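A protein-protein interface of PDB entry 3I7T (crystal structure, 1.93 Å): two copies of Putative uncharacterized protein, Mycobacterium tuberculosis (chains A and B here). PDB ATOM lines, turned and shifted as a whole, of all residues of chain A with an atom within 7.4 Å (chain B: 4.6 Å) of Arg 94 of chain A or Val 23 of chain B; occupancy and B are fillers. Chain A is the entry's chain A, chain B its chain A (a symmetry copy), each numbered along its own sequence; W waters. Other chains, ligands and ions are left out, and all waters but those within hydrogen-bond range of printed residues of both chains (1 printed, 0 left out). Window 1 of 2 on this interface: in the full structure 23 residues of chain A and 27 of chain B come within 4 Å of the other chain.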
ATOM      1  N   LEU A  63     -30.747 -32.944  19.923  1.00  0.00           N
ATOM      2  CA  LEU A  63     -30.065 -31.716  20.346  1.00  0.00           C
ATOM      3  C   LEU A  63     -29.718 -31.705  21.836  1.00  0.00           C
ATOM      4  O   LEU A  63     -28.709 -31.126  22.233  1.00  0.00           O
ATOM      5  CB  LEU A  63     -30.906 -30.490  20.000  1.00  0.00           C
ATOM      6  CG  LEU A  63     -31.010 -30.292  18.492  1.00  0.00           C
ATOM      7  CD1 LEU A  63     -32.059 -29.230  18.163  1.00  0.00           C
ATOM      8  CD2 LEU A  63     -29.639 -29.904  17.940  1.00  0.00           C
ATOM      9  N   ASP A  65     -28.487 -33.868  23.499  1.00  0.00           N
ATOM     10  CA  ASP A  65     -27.251 -34.621  23.758  1.00  0.00           C
ATOM     11  C   ASP A  65     -25.989 -33.814  23.426  1.00  0.00           C
ATOM     12  O   ASP A  65     -24.870 -34.204  23.792  1.00  0.00           O
ATOM     13  CB  ASP A  65     -27.223 -35.942  22.981  1.00  0.00           C
ATOM     14  CG  ASP A  65     -28.281 -36.905  23.424  1.00  0.00           C
ATOM     15  OD1 ASP A  65     -28.447 -37.089  24.642  1.00  0.00           O
ATOM     16  OD2 ASP A  65     -28.937 -37.494  22.543  1.00  0.00           O
ATOM     17  N   VAL A  66     -26.179 -32.708  22.714  1.00  0.00           N
ATOM     18  CA  VAL A  66     -25.072 -31.875  22.245  1.00  0.00           C
ATOM     19  C   VAL A  66     -24.329 -31.197  23.422  1.00  0.00           C
ATOM     20  O   VAL A  66     -24.950 -30.537  24.264  1.00  0.00           O
ATOM     21  CB  VAL A  66     -25.591 -30.828  21.227  1.00  0.00           C
ATOM     22  CG1 VAL A  66     -24.513 -29.771  20.925  1.00  0.00           C
ATOM     23  CG2 VAL A  66     -26.088 -31.533  19.963  1.00  0.00           C
ATOM     24  N   VAL A  67     -23.017 -31.399  23.505  1.00  0.00           N
ATOM     25  CA  VAL A  67     -22.235 -30.830  24.599  1.00  0.00           C
ATOM     26  C   VAL A  67     -21.389 -29.674  24.096  1.00  0.00           C
ATOM     27  O   VAL A  67     -20.966 -28.815  24.883  1.00  0.00           O
ATOM     28  CB  VAL A  67     -21.307 -31.874  25.291  1.00  0.00           C
ATOM     29  CG1 VAL A  67     -22.138 -32.970  26.020  1.00  0.00           C
ATOM     30  CG2 VAL A  67     -20.330 -32.491  24.288  1.00  0.00           C
ATOM     31  N   ARG A  68     -21.128 -29.667  22.793  1.00  0.00           N
ATOM     32  CA  ARG A  68     -20.348 -28.594  22.175  1.00  0.00           C
ATOM     33  C   ARG A  68     -20.827 -28.238  20.772  1.00  0.00           C
ATOM     34  O   ARG A  68     -21.099 -29.123  19.951  1.00  0.00           O
ATOM     35  CB  ARG A  68     -18.849 -28.943  22.116  1.00  0.00           C
ATOM     36  CG  ARG A  68     -18.035 -27.847  21.383  1.00  0.00           C
ATOM     37  CD  ARG A  68     -16.572 -28.216  21.058  1.00  0.00           C
ATOM     38  NE  ARG A  68     -15.734 -28.561  22.211  1.00  0.00           N
ATOM     39  CZ  ARG A  68     -15.077 -27.678  22.969  1.00  0.00           C
ATOM     40  NH1 ARG A  68     -15.188 -26.367  22.751  1.00  0.00           N
ATOM     41  NH2 ARG A  68     -14.321 -28.100  23.974  1.00  0.00           N
ATOM     42  N   HIS A  86     -29.139 -19.810  17.750  1.00  0.00           N
ATOM     43  CA  HIS A  86     -28.475 -20.819  18.569  1.00  0.00           C
ATOM     44  C   HIS A  86     -29.192 -20.891  19.918  1.00  0.00           C
ATOM     45  O   HIS A  86     -29.395 -21.979  20.485  1.00  0.00           O
ATOM     46  CB  HIS A  86     -26.987 -20.435  18.750  1.00  0.00           C
ATOM     47  CG  HIS A  86     -26.154 -21.485  19.429  1.00  0.00           C
ATOM     48  ND1 HIS A  86     -26.075 -21.602  20.803  1.00  0.00           N
ATOM     49  CD2 HIS A  86     -25.351 -22.453  18.924  1.00  0.00           C
ATOM     50  CE1 HIS A  86     -25.265 -22.599  21.115  1.00  0.00           C
ATOM     51  NE2 HIS A  86     -24.821 -23.141  19.990  1.00  0.00           N
ATOM     52  N   ALA A  89     -32.479 -22.618  19.781  1.00  0.00           N
ATOM     53  CA  ALA A  89     -32.231 -24.059  19.733  1.00  0.00           C
ATOM     54  C   ALA A  89     -31.682 -24.603  21.068  1.00  0.00           C
ATOM     55  O   ALA A  89     -32.042 -25.703  21.497  1.00  0.00           O
ATOM     56  CB  ALA A  89     -31.288 -24.405  18.568  1.00  0.00           C
ATOM     57  N   PHE A  90     -30.839 -23.828  21.748  1.00  0.00           N
ATOM     58  CA  PHE A  90     -30.091 -24.377  22.885  1.00  0.00           C
ATOM     59  C   PHE A  90     -30.219 -23.632  24.216  1.00  0.00           C
ATOM     60  O   PHE A  90     -29.379 -23.798  25.094  1.00  0.00           O
ATOM     61  CB  PHE A  90     -28.607 -24.476  22.539  1.00  0.00           C
ATOM     62  CG  PHE A  90     -28.278 -25.498  21.481  1.00  0.00           C
ATOM     63  CD1 PHE A  90     -28.336 -26.860  21.762  1.00  0.00           C
ATOM     64  CD2 PHE A  90     -27.857 -25.089  20.221  1.00  0.00           C
ATOM     65  CE1 PHE A  90     -27.996 -27.809  20.800  1.00  0.00           C
ATOM     66  CE2 PHE A  90     -27.515 -26.016  19.254  1.00  0.00           C
ATOM     67  CZ  PHE A  90     -27.583 -27.394  19.544  1.00  0.00           C
ATOM     68  N   GLY A  91     -31.262 -22.827  24.372  1.00  0.00           N
ATOM     69  CA  GLY A  91     -31.453 -22.061  25.592  1.00  0.00           C
ATOM     70  C   GLY A  91     -31.499 -22.896  26.858  1.00  0.00           C
ATOM     71  O   GLY A  91     -30.972 -22.482  27.896  1.00  0.00           O
ATOM     72  N   LYS A  92     -32.131 -24.064  26.791  1.00  0.00           N
ATOM     73  CA  LYS A  92     -32.186 -24.953  27.961  1.00  0.00           C
ATOM     74  C   LYS A  92     -30.952 -25.853  28.022  1.00  0.00           C
ATOM     75  O   LYS A  92     -30.337 -26.025  29.077  1.00  0.00           O
ATOM     76  CB  LYS A  92     -33.437 -25.824  27.913  1.00  0.00           C
ATOM     77  CG  LYS A  92     -34.688 -25.093  27.451  1.00  0.00           C
ATOM     78  CD  LYS A  92     -35.737 -26.053  26.861  1.00  0.00           C
ATOM     79  CE  LYS A  92     -35.296 -26.635  25.504  1.00  0.00           C
ATOM     80  NZ  LYS A  92     -34.365 -27.787  25.631  1.00  0.00           N
ATOM     81  N   ILE A  93     -30.596 -26.412  26.875  1.00  0.00           N
ATOM     82  CA  ILE A  93     -29.509 -27.379  26.764  1.00  0.00           C
ATOM     83  C   ILE A  93     -28.133 -26.774  27.083  1.00  0.00           C
ATOM     84  O   ILE A  93     -27.372 -27.306  27.915  1.00  0.00           O
ATOM     85  CB  ILE A  93     -29.528 -28.012  25.363  1.00  0.00           C
ATOM     86  CG1 ILE A  93     -30.889 -28.703  25.135  1.00  0.00           C
ATOM     87  CG2 ILE A  93     -28.346 -28.954  25.189  1.00  0.00           C
ATOM     88  CD1 ILE A  93     -31.385 -28.709  23.660  1.00  0.00           C
ATOM     89  N   ARG A  94     -27.827 -25.687  26.421  1.00  0.00           N
ATOM     90  CA  ARG A  94     -26.657 -24.895  26.706  1.00  0.00           C
ATOM     91  C   ARG A  94     -25.344 -25.677  26.586  1.00  0.00           C
ATOM     92  O   ARG A  94     -24.636 -25.809  27.545  1.00  0.00           O
ATOM     93  CB  ARG A  94     -26.759 -24.302  28.078  1.00  0.00           C
ATOM     94  CG  ARG A  94     -27.392 -23.075  28.096  1.00  0.00           C
ATOM     95  CD  ARG A  94     -28.138 -22.931  29.292  1.00  0.00           C
ATOM     96  N   PRO A  95     -25.046 -26.179  25.414  1.00  0.00           N
ATOM     97  CA  PRO A  95     -23.742 -26.760  25.201  1.00  0.00           C
ATOM     98  C   PRO A  95     -22.724 -25.625  25.299  1.00  0.00           C
ATOM     99  O   PRO A  95     -23.118 -24.457  25.329  1.00  0.00           O
ATOM    100  CB  PRO A  95     -23.836 -27.254  23.755  1.00  0.00           C
ATOM    101  CG  PRO A  95     -24.710 -26.219  23.084  1.00  0.00           C
ATOM    102  CD  PRO A  95     -25.730 -25.850  24.147  1.00  0.00           C
ATOM    103  N   VAL A  96     -21.435 -25.937  25.374  1.00  0.00           N
ATOM    104  CA  VAL A  96     -20.421 -24.881  25.219  1.00  0.00           C
ATOM    105  C   VAL A  96     -20.347 -24.500  23.739  1.00  0.00           C
ATOM    106  O   VAL A  96     -20.711 -25.303  22.878  1.00  0.00           O
ATOM    107  CB  VAL A  96     -19.044 -25.339  25.723  1.00  0.00           C
ATOM    108  CG1 VAL A  96     -19.184 -25.979  27.128  1.00  0.00           C
ATOM    109  CG2 VAL A  96     -18.400 -26.318  24.711  1.00  0.00           C
ATOM    110  N   THR A  97     -19.941 -23.269  23.423  1.00  0.00           N
ATOM    111  CA  THR A  97     -19.648 -22.937  22.028  1.00  0.00           C
ATOM    112  C   THR A  97     -18.425 -22.080  21.890  1.00  0.00           C
ATOM    113  O   THR A  97     -17.851 -21.612  22.875  1.00  0.00           O
ATOM    114  CB  THR A  97     -20.669 -22.003  21.331  1.00  0.00           C
ATOM    115  OG1 THR A  97     -21.754 -21.645  22.186  1.00  0.00           O
ATOM    116  CG2 THR A  97     -21.126 -22.550  20.013  1.00  0.00           C
ATOM    117  N   ARG B   4     -25.458 -34.982  33.609  1.00  0.00           N
ATOM    118  CA  ARG B   4     -24.825 -33.811  33.009  1.00  0.00           C
ATOM    119  C   ARG B   4     -24.754 -32.609  33.955  1.00  0.00           C
ATOM    120  O   ARG B   4     -25.738 -32.252  34.592  1.00  0.00           O
ATOM    121  CB  ARG B   4     -25.572 -33.433  31.724  1.00  0.00           C
ATOM    122  CG  ARG B   4     -25.023 -32.213  30.949  1.00  0.00           C
ATOM    123  CD  ARG B   4     -25.770 -32.079  29.614  1.00  0.00           C
ATOM    124  NE  ARG B   4     -25.492 -30.825  28.920  1.00  0.00           N
ATOM    125  CZ  ARG B   4     -25.474 -30.703  27.596  1.00  0.00           C
ATOM    126  NH1 ARG B   4     -25.205 -29.529  27.038  1.00  0.00           N
ATOM    127  NH2 ARG B   4     -25.727 -31.766  26.832  1.00  0.00           N
ATOM    128  N   THR B   5     -23.583 -31.986  34.035  1.00  0.00           N
ATOM    129  CA  THR B   5     -23.423 -30.782  34.829  1.00  0.00           C
ATOM    130  C   THR B   5     -22.839 -29.676  33.965  1.00  0.00           C
ATOM    131  O   THR B   5     -22.036 -29.932  33.065  1.00  0.00           O
ATOM    132  CB  THR B   5     -22.528 -31.011  36.087  1.00  0.00           C
ATOM    133  OG1 THR B   5     -21.386 -31.787  35.730  1.00  0.00           O
ATOM    134  CG2 THR B   5     -23.275 -31.761  37.156  1.00  0.00           C
ATOM    135  N   MET B   6     -23.246 -28.445  34.250  1.00  0.00           N
ATOM    136  CA  MET B   6     -22.856 -27.303  33.448  1.00  0.00           C
ATOM    137  C   MET B   6     -22.417 -26.136  34.304  1.00  0.00           C
ATOM    138  O   MET B   6     -22.926 -25.922  35.415  1.00  0.00           O
ATOM    139  CB  MET B   6     -24.016 -26.884  32.556  1.00  0.00           C
ATOM    140  CG  MET B   6     -24.567 -28.036  31.759  1.00  0.00           C
ATOM    141  SD  MET B   6     -25.860 -27.583  30.594  1.00  0.00           S
ATOM    142  CE  MET B   6     -27.041 -26.739  31.643  1.00  0.00           C
ATOM    143  N   GLY B  18     -26.919 -18.656  24.444  1.00  0.00           N
ATOM    144  CA  GLY B  18     -27.413 -19.915  25.011  1.00  0.00           C
ATOM    145  C   GLY B  18     -26.340 -20.991  24.999  1.00  0.00           C
ATOM    146  O   GLY B  18     -26.425 -21.957  24.223  1.00  0.00           O
ATOM    147  N   TYR B  19     -25.317 -20.810  25.830  1.00  0.00           N
ATOM    148  CA  TYR B  19     -24.189 -21.750  25.904  1.00  0.00           C
ATOM    149  C   TYR B  19     -23.601 -21.731  27.327  1.00  0.00           C
ATOM    150  O   TYR B  19     -23.853 -20.798  28.096  1.00  0.00           O
ATOM    151  CB  TYR B  19     -23.111 -21.418  24.852  1.00  0.00           C
ATOM    152  CG  TYR B  19     -22.153 -20.281  25.223  1.00  0.00           C
ATOM    153  CD1 TYR B  19     -20.948 -20.548  25.873  1.00  0.00           C
ATOM    154  CD2 TYR B  19     -22.448 -18.947  24.901  1.00  0.00           C
ATOM    155  CE1 TYR B  19     -20.064 -19.523  26.218  1.00  0.00           C
ATOM    156  CE2 TYR B  19     -21.573 -17.914  25.232  1.00  0.00           C
ATOM    157  CZ  TYR B  19     -20.377 -18.205  25.894  1.00  0.00           C
ATOM    158  OH  TYR B  19     -19.492 -17.185  26.232  1.00  0.00           O
ATOM    159  N   SER B  20     -22.828 -22.763  27.667  1.00  0.00           N
ATOM    160  CA  SER B  20     -22.199 -22.880  28.975  1.00  0.00           C
ATOM    161  C   SER B  20     -20.701 -22.666  28.875  1.00  0.00           C
ATOM    162  O   SER B  20     -20.098 -22.892  27.833  1.00  0.00           O
ATOM    163  CB  SER B  20     -22.444 -24.270  29.567  1.00  0.00           C
ATOM    164  OG  SER B  20     -23.806 -24.492  29.837  1.00  0.00           O
ATOM    165  N   ALA B  22     -18.584 -24.483  30.675  1.00  0.00           N
ATOM    166  CA  ALA B  22     -18.114 -25.865  30.643  1.00  0.00           C
ATOM    167  C   ALA B  22     -19.268 -26.847  30.815  1.00  0.00           C
ATOM    168  O   ALA B  22     -20.252 -26.550  31.503  1.00  0.00           O
ATOM    169  CB  ALA B  22     -17.079 -26.101  31.710  1.00  0.00           C
ATOM    170  N   VAL B  23     -19.139 -28.017  30.197  1.00  0.00           N
ATOM    171  CA  VAL B  23     -20.099 -29.089  30.406  1.00  0.00           C
ATOM    172  C   VAL B  23     -19.335 -30.369  30.679  1.00  0.00           C
ATOM    173  O   VAL B  23     -18.327 -30.635  30.023  1.00  0.00           O
ATOM    174  CB  VAL B  23     -21.030 -29.257  29.176  1.00  0.00           C
ATOM    175  CG1 VAL B  23     -22.012 -30.429  29.381  1.00  0.00           C
ATOM    176  CG2 VAL B  23     -21.790 -27.973  28.947  1.00  0.00           C
ATOM    177  N   ARG B  24     -19.805 -31.136  31.667  1.00  0.00           N
ATOM    178  CA  ARG B  24     -19.256 -32.450  32.009  1.00  0.00           C
ATOM    179  C   ARG B  24     -20.349 -33.539  31.902  1.00  0.00           C
ATOM    180  O   ARG B  24     -21.440 -33.361  32.430  1.00  0.00           O
ATOM    181  CB  ARG B  24     -18.665 -32.427  33.437  1.00  0.00           C
ATOM    182  CG  ARG B  24     -18.321 -33.832  33.995  1.00  0.00           C
ATOM    183  CD  ARG B  24     -17.708 -33.784  35.398  1.00  0.00           C
ATOM    184  NE  ARG B  24     -17.075 -35.059  35.775  1.00  0.00           N
ATOM    185  CZ  ARG B  24     -16.062 -35.159  36.630  1.00  0.00           C
ATOM    186  NH1 ARG B  24     -15.559 -34.065  37.202  1.00  0.00           N
ATOM    187  NH2 ARG B  24     -15.537 -36.343  36.905  1.00  0.00           N
ATOM    188  N   ILE B  25     -20.074 -34.622  31.171  1.00  0.00           N
ATOM    189  CA  ILE B  25     -20.872 -35.857  31.243  1.00  0.00           C
ATOM    190  C   ILE B  25     -19.907 -37.019  31.189  1.00  0.00           C
ATOM    191  O   ILE B  25     -19.002 -37.028  30.377  1.00  0.00           O
ATOM    192  CB  ILE B  25     -21.830 -36.094  30.042  1.00  0.00           C
ATOM    193  CG1 ILE B  25     -21.992 -34.856  29.194  1.00  0.00           C
ATOM    194  CG2 ILE B  25     -23.140 -36.791  30.469  1.00  0.00           C
ATOM    195  CD1 ILE B  25     -20.964 -34.842  28.088  1.00  0.00           C
ATOM    196  N   LEU B  28     -15.752 -36.873  30.427  1.00  0.00           N
ATOM    197  CA  LEU B  28     -15.544 -35.729  29.541  1.00  0.00           C
ATOM    198  C   LEU B  28     -15.945 -34.390  30.154  1.00  0.00           C
ATOM    199  O   LEU B  28     -17.044 -34.255  30.697  1.00  0.00           O
ATOM    200  CB  LEU B  28     -16.360 -35.923  28.268  1.00  0.00           C
ATOM    201  CG  LEU B  28     -16.081 -34.899  27.177  1.00  0.00           C
ATOM    202  CD1 LEU B  28     -14.589 -34.965  26.797  1.00  0.00           C
ATOM    203  CD2 LEU B  28     -16.981 -35.132  25.947  1.00  0.00           C
ATOM    204  N   VAL B  29     -15.051 -33.406  30.039  1.00  0.00           N
ATOM    205  CA  VAL B  29     -15.377 -31.994  30.289  1.00  0.00           C
ATOM    206  C   VAL B  29     -14.953 -31.181  29.062  1.00  0.00           C
ATOM    207  O   VAL B  29     -13.777 -31.210  28.661  1.00  0.00           O
ATOM    208  CB  VAL B  29     -14.682 -31.458  31.543  1.00  0.00           C
ATOM    209  CG1 VAL B  29     -15.054 -30.015  31.786  1.00  0.00           C
ATOM    210  CG2 VAL B  29     -15.062 -32.309  32.768  1.00  0.00           C
ATOM    211  N   VAL B  30     -15.910 -30.496  28.439  1.00  0.00           N
ATOM    212  CA  VAL B  30     -15.576 -29.537  27.380  1.00  0.00           C
ATOM    213  C   VAL B  30     -15.725 -28.093  27.854  1.00  0.00           C
ATOM    214  O   VAL B  30     -16.625 -27.766  28.623  1.00  0.00           O
ATOM    215  CB  VAL B  30     -16.410 -29.770  26.096  1.00  0.00           C
ATOM    216  CG1 VAL B  30     -16.098 -31.138  25.539  1.00  0.00           C
ATOM    217  CG2 VAL B  30     -17.885 -29.636  26.383  1.00  0.00           C
HETATM  218  O   HOH W   1     -28.588 -29.559  29.163  1.00  0.00           O
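Water W1 lies within hydrogen-bond range of the backbone carbonyl oxygen (O) of Ile 93 of chain A, the guanidinium group (NE) of Arg 4 of chain B and the side-chain sulfur (SD) of Met 6 of chain B.
No position is printed for both chains.
Of the 25 pairs that touch across the chains among the printed residues, none has its exchanged pair printed and touching as well.
Val 30 of chain B touches Arg 68 of chain A (CB to NH2, 3.4 Å).
O of Phe 90 of chain A touches O of Gly 18 of chain B (3.6 Å).
CA of Arg 94 of chain A touches O of Gly 18 of chain B (3.9 Å).
O of Arg 94 of chain A touches CG2 of Val 23 of chain B, 3.8 Å away.
NH1 of Arg 4 of chain B touches CA of Pro 95 of chain A, 3.6 Å away.
Pro 95 of chain A touches Gly 18 of chain B.
Pro 95 of chain A touches Tyr 19 of chain B (O to CA, 3.0 Å).
CG1 of Val 96 of chain A touches O of Ser 20 of chain B (3.3 Å).
Val 30 of chain B touches Val 96 of chain A.
Tyr 19 of chain B touches Thr 97 of chain A (CB to OG1, 3.0 Å).
Of the printed residues of chain B, Val 66 of chain A touches Arg 4.
Of the printed residues of chain B, His 86 of chain A touches Gly 18 (3.4 Å).
Arg 94 of chain A touches six residues of chain B.
Of the printed residues of chain A, Met 6 of chain B touches Ile 93 (3.1 Å) and Arg 94 (3.7 Å).
Printed residues of chain A within 4 Å of Val 30 of chain B: Val 67 (3.5 Å), Arg 68 (3.4 Å) and Val 96 (3.5 Å).
N of Val 96 of chain A sits at hydrogen-bond distance from O of Val 67 of chain A, at 3.0 Å.
NE of Arg 4 of chain B sits at hydrogen-bond distance from SD of Met 6 of chain B (3.7 Å).
The side-chain sulfur (SD) of Met 6 of chain B sits close to the side-chain hydroxyl (OG) of Ser 20 of chain B, 3.8 Å away.
The backbone NH of Val 30 of chain B is in hydrogen-bond range of the backbone carbonyl oxygen of Val 23 of chain B (2.9 Å).
The guanidinium group (NH2) of Arg 4 of chain B is in hydrogen-bond range of the backbone carbonyl oxygen (O) of Val 66 of chain A, at 3.0 Å.
A ring nitrogen (ND1) of His 86 of chain A sits close to the backbone carbonyl oxygen (O) of Gly 18 of chain B.
NH1 of Arg 4 of chain B sits at hydrogen-bond distance from O of Ile 93 of chain A (3.2 Å).
O of Arg 94 of chain A is in hydrogen-bond range of OG of Ser 20 of chain B (2.8 Å).
The backbone carbonyl oxygen of Pro 95 of chain A lies within hydrogen-bond range of the backbone NH of Ser 20 of chain B (2.9 Å).
O of Ile 93 of chain A lies close to SD of Met 6 of chain B, at 3.1 Å.
The side-chain sulfur of Met 6 of chain B sits close to the backbone carbonyl oxygen of Arg 94 of chain A (3.7 Å).
Hydrophobic or aromatic side chains of chain B within 4 Å of the printed part of chain A: Met 6, Tyr 19, Val 23, Ile 25 and Val 30.
Along chain B the printed residues that touch a printed residue of chain A span positions 4 to 30.
Hydrophobic or aromatic side chains of chain A that line the printed part of chain B: Val 67, His 86, Phe 90, Ile 93, Pro 95 and Val 96.
Among the printed residues, 25 pairs touch across the chains.
Among the printed residues, no Asp or Glu carboxylate lies within 4 Å of a Lys or Arg side-chain nitrogen of the other chain.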
